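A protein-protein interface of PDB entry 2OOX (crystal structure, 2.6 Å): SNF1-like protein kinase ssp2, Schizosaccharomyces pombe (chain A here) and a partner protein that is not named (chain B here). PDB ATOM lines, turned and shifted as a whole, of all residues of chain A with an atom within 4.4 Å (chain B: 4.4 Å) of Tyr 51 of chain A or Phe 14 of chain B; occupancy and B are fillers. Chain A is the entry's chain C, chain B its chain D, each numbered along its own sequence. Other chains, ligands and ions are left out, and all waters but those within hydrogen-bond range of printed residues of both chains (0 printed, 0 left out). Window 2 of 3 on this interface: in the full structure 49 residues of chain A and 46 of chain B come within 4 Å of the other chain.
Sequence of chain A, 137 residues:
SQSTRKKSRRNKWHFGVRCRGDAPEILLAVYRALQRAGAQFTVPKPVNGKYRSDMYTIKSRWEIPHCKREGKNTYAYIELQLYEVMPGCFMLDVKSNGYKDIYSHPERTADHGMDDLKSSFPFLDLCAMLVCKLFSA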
ATOM      1  N   PRO A  44      -3.481  15.375  -2.275  1.00  0.00           N
ATOM      2  CA  PRO A  44      -3.639  16.598  -1.486  1.00  0.00           C
ATOM      3  C   PRO A  44      -4.022  17.804  -2.365  1.00  0.00           C
ATOM      4  O   PRO A  44      -3.768  17.799  -3.591  1.00  0.00           O
ATOM      5  CB  PRO A  44      -2.257  16.796  -0.853  1.00  0.00           C
ATOM      6  CG  PRO A  44      -1.386  15.680  -1.376  1.00  0.00           C
ATOM      7  CD  PRO A  44      -2.067  15.083  -2.555  1.00  0.00           C
ATOM      8  N   PRO A  46      -3.728  22.197  -2.450  1.00  0.00           N
ATOM      9  CA  PRO A  46      -3.061  23.385  -1.899  1.00  0.00           C
ATOM     10  C   PRO A  46      -4.014  24.553  -1.555  1.00  0.00           C
ATOM     11  O   PRO A  46      -4.973  24.800  -2.305  1.00  0.00           O
ATOM     12  CB  PRO A  46      -2.083  23.789  -3.012  1.00  0.00           C
ATOM     13  CG  PRO A  46      -2.249  22.756  -4.136  1.00  0.00           C
ATOM     14  CD  PRO A  46      -3.559  22.101  -3.913  1.00  0.00           C
ATOM     15  N   LYS A  50       0.190  26.626  -1.817  1.00  0.00           N
ATOM     16  CA  LYS A  50       0.812  26.224  -0.539  1.00  0.00           C
ATOM     17  C   LYS A  50       0.072  25.019   0.095  1.00  0.00           C
ATOM     18  O   LYS A  50      -1.105  24.802  -0.200  1.00  0.00           O
ATOM     19  CB  LYS A  50       0.837  27.405   0.426  1.00  0.00           C
ATOM     20  N   TYR A  51       0.744  24.240   0.956  1.00  0.00           N
ATOM     21  CA  TYR A  51       0.145  22.999   1.482  1.00  0.00           C
ATOM     22  C   TYR A  51      -0.193  23.027   2.948  1.00  0.00           C
ATOM     23  O   TYR A  51       0.338  23.836   3.702  1.00  0.00           O
ATOM     24  CB  TYR A  51       1.044  21.802   1.241  1.00  0.00           C
ATOM     25  CG  TYR A  51       1.106  21.385  -0.190  1.00  0.00           C
ATOM     26  CD1 TYR A  51       2.147  21.816  -1.003  1.00  0.00           C
ATOM     27  CD2 TYR A  51       0.132  20.553  -0.738  1.00  0.00           C
ATOM     28  CE1 TYR A  51       2.223  21.430  -2.315  1.00  0.00           C
ATOM     29  CE2 TYR A  51       0.202  20.161  -2.072  1.00  0.00           C
ATOM     30  CZ  TYR A  51       1.256  20.608  -2.849  1.00  0.00           C
ATOM     31  OH  TYR A  51       1.355  20.257  -4.166  1.00  0.00           O
ATOM     32  N   ARG A  52      -1.083  22.121   3.344  1.00  0.00           N
ATOM     33  CA  ARG A  52      -1.441  21.945   4.744  1.00  0.00           C
ATOM     34  C   ARG A  52      -1.180  20.491   5.182  1.00  0.00           C
ATOM     35  O   ARG A  52      -1.283  19.559   4.372  1.00  0.00           O
ATOM     36  CB  ARG A  52      -2.910  22.327   5.002  1.00  0.00           C
ATOM     37  CG  ARG A  52      -3.509  23.420   4.088  1.00  0.00           C
ATOM     38  CD  ARG A  52      -4.837  24.009   4.643  1.00  0.00           C
ATOM     39  NE  ARG A  52      -4.655  24.747   5.902  1.00  0.00           N
ATOM     40  CZ  ARG A  52      -4.093  25.956   6.019  1.00  0.00           C
ATOM     41  NH1 ARG A  52      -3.644  26.610   4.945  1.00  0.00           N
ATOM     42  NH2 ARG A  52      -3.970  26.523   7.221  1.00  0.00           N
ATOM     43  N   MET A  55      -2.222  16.943   4.198  1.00  0.00           N
ATOM     44  CA  MET A  55      -1.431  16.251   3.172  1.00  0.00           C
ATOM     45  C   MET A  55      -1.189  14.784   3.570  1.00  0.00           C
ATOM     46  O   MET A  55      -1.211  13.878   2.731  1.00  0.00           O
ATOM     47  CB  MET A  55      -0.096  16.975   3.093  1.00  0.00           C
ATOM     48  CG  MET A  55       0.649  16.917   1.802  1.00  0.00           C
ATOM     49  SD  MET A  55       2.243  17.727   2.053  1.00  0.00           S
ATOM     50  CE  MET A  55       3.232  16.796   0.875  1.00  0.00           C
ATOM     51  N   PRO B  12       0.691  11.893  -6.967  1.00  0.00           N
ATOM     52  CA  PRO B  12       0.786  13.336  -7.103  1.00  0.00           C
ATOM     53  C   PRO B  12       2.088  13.792  -7.776  1.00  0.00           C
ATOM     54  O   PRO B  12       3.151  13.219  -7.511  1.00  0.00           O
ATOM     55  CB  PRO B  12       0.740  13.802  -5.655  1.00  0.00           C
ATOM     56  CG  PRO B  12      -0.175  12.815  -5.002  1.00  0.00           C
ATOM     57  CD  PRO B  12       0.097  11.500  -5.678  1.00  0.00           C
ATOM     58  N   ALA B  13       1.985  14.808  -8.642  1.00  0.00           N
ATOM     59  CA  ALA B  13       3.097  15.280  -9.489  1.00  0.00           C
ATOM     60  C   ALA B  13       4.316  15.711  -8.673  1.00  0.00           C
ATOM     61  O   ALA B  13       5.415  15.200  -8.872  1.00  0.00           O
ATOM     62  CB  ALA B  13       2.627  16.404 -10.413  1.00  0.00           C
ATOM     63  N   PHE B  14       4.111  16.652  -7.756  1.00  0.00           N
ATOM     64  CA  PHE B  14       5.082  16.940  -6.711  1.00  0.00           C
ATOM     65  C   PHE B  14       5.285  15.615  -5.966  1.00  0.00           C
ATOM     66  O   PHE B  14       4.435  14.729  -6.049  1.00  0.00           O
ATOM     67  CB  PHE B  14       4.532  18.037  -5.786  1.00  0.00           C
ATOM     68  CG  PHE B  14       3.500  17.547  -4.788  1.00  0.00           C
ATOM     69  CD1 PHE B  14       3.710  17.712  -3.423  1.00  0.00           C
ATOM     70  CD2 PHE B  14       2.332  16.913  -5.206  1.00  0.00           C
ATOM     71  CE1 PHE B  14       2.772  17.257  -2.495  1.00  0.00           C
ATOM     72  CE2 PHE B  14       1.399  16.454  -4.283  1.00  0.00           C
ATOM     73  CZ  PHE B  14       1.623  16.623  -2.928  1.00  0.00           C
ATOM     74  N   LEU B  15       6.386  15.462  -5.242  1.00  0.00           N
ATOM     75  CA  LEU B  15       6.740  14.167  -4.611  1.00  0.00           C
ATOM     76  C   LEU B  15       7.549  13.316  -5.593  1.00  0.00           C
ATOM     77  O   LEU B  15       8.625  12.819  -5.254  1.00  0.00           O
ATOM     78  CB  LEU B  15       5.516  13.372  -4.103  1.00  0.00           C
ATOM     79  CG  LEU B  15       4.512  13.891  -3.065  1.00  0.00           C
ATOM     80  CD1 LEU B  15       3.411  12.870  -2.840  1.00  0.00           C
ATOM     81  CD2 LEU B  15       5.178  14.239  -1.754  1.00  0.00           C
ATOM     82  N   THR B  16       7.033  13.152  -6.809  1.00  0.00           N
ATOM     83  CA  THR B  16       7.817  12.565  -7.890  1.00  0.00           C
ATOM     84  C   THR B  16       8.749  13.661  -8.392  1.00  0.00           C
ATOM     85  O   THR B  16       9.553  14.195  -7.627  1.00  0.00           O
ATOM     86  CB  THR B  16       6.932  12.039  -9.054  1.00  0.00           C
ATOM     87  OG1 THR B  16       6.078  13.090  -9.521  1.00  0.00           O
ATOM     88  CG2 THR B  16       6.075  10.859  -8.610  1.00  0.00           C
ATOM     89  N   LEU B  23       8.050  22.759  -1.013  1.00  0.00           N
ATOM     90  CA  LEU B  23       7.637  24.145  -1.196  1.00  0.00           C
ATOM     91  C   LEU B  23       7.970  24.749   0.168  1.00  0.00           C
ATOM     92  O   LEU B  23       8.973  25.447   0.311  1.00  0.00           O
ATOM     93  CB  LEU B  23       6.151  24.269  -1.557  1.00  0.00           C
ATOM     94  CG  LEU B  23       5.635  23.616  -2.855  1.00  0.00           C
ATOM     95  CD1 LEU B  23       4.497  24.439  -3.430  1.00  0.00           C
ATOM     96  CD2 LEU B  23       6.702  23.417  -3.944  1.00  0.00           C
ATOM     97  N   LEU B  25       6.365  22.371   2.484  1.00  0.00           N
ATOM     98  CA  LEU B  25       5.931  21.041   2.891  1.00  0.00           C
ATOM     99  C   LEU B  25       5.901  20.939   4.419  1.00  0.00           C
ATOM    100  O   LEU B  25       6.920  21.066   5.100  1.00  0.00           O
ATOM    101  CB  LEU B  25       6.748  19.937   2.196  1.00  0.00           C
ATOM    102  CG  LEU B  25       6.236  19.490   0.807  1.00  0.00           C
ATOM    103  CD1 LEU B  25       5.495  20.567  -0.009  1.00  0.00           C
ATOM    104  CD2 LEU B  25       7.332  18.852  -0.052  1.00  0.00           C
ATOM    105  N   PRO B  26       4.710  20.751   4.969  1.00  0.00           N
ATOM    106  CA  PRO B  26       4.638  20.762   6.411  1.00  0.00           C
ATOM    107  C   PRO B  26       4.939  19.406   7.016  1.00  0.00           C
ATOM    108  O   PRO B  26       5.049  18.403   6.310  1.00  0.00           O
ATOM    109  CB  PRO B  26       3.192  21.157   6.683  1.00  0.00           C
ATOM    110  CG  PRO B  26       2.437  20.757   5.433  1.00  0.00           C
ATOM    111  CD  PRO B  26       3.407  20.516   4.330  1.00  0.00           C
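Of the 6 printed residues of chain A, 4 touch a printed residue of chain B. Printed residues of chain B that touch a printed residue of chain A: Pro 12, Phe 14, Leu 23, Leu 25 and Pro 26. Among the printed residues, no Asp or Glu carboxylate lies within 4 Å of a Lys or Arg side-chain nitrogen of the other chain.
Of the printed residues of chain B, Tyr 51 of chain A touches Phe 14 (3.5 Å), Leu 23 (3.9 Å) and Leu 25 (3.7 Å). Phe 14 of chain B touches just these residues of chain A: Pro 44, Tyr 51 and Met 55. Leu 15 of chain B touches none of the printed residues of chain A. Of the printed residues of chain A, Leu 23 of chain B touches Tyr 51 (3.9 Å). Of the printed residues of chain A, Pro 26 of chain B touches Arg 52 (3.6 Å) and Met 55 (3.8 Å). The nearest residue of chain B that does not touch Tyr 51 of chain A is Pro 26 of chain B (4.1 Å). The nearest printed residue of chain A that does not touch Phe 14 of chain B is Pro 46 of chain A (7.3 Å).
Pro 12 of chain B touches Pro 44 of chain A. Pro 44 of chain A touches Phe 14 of chain B (CG to CZ, 3.5 Å). Tyr 51 of chain A touches Phe 14 of chain B (OH to CG, 3.5 Å). Tyr 51 of chain A touches Leu 23 of chain B. Leu 25 of chain B touches Tyr 51 of chain A (CD1 to CD1, 3.7 Å). C of Arg 52 of chain A touches CG of Pro 26 of chain B, 3.6 Å away. Phe 14 of chain B touches Met 55 of chain A (CE1 to CE, 3.4 Å). Met 55 of chain A touches Pro 26 of chain B.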
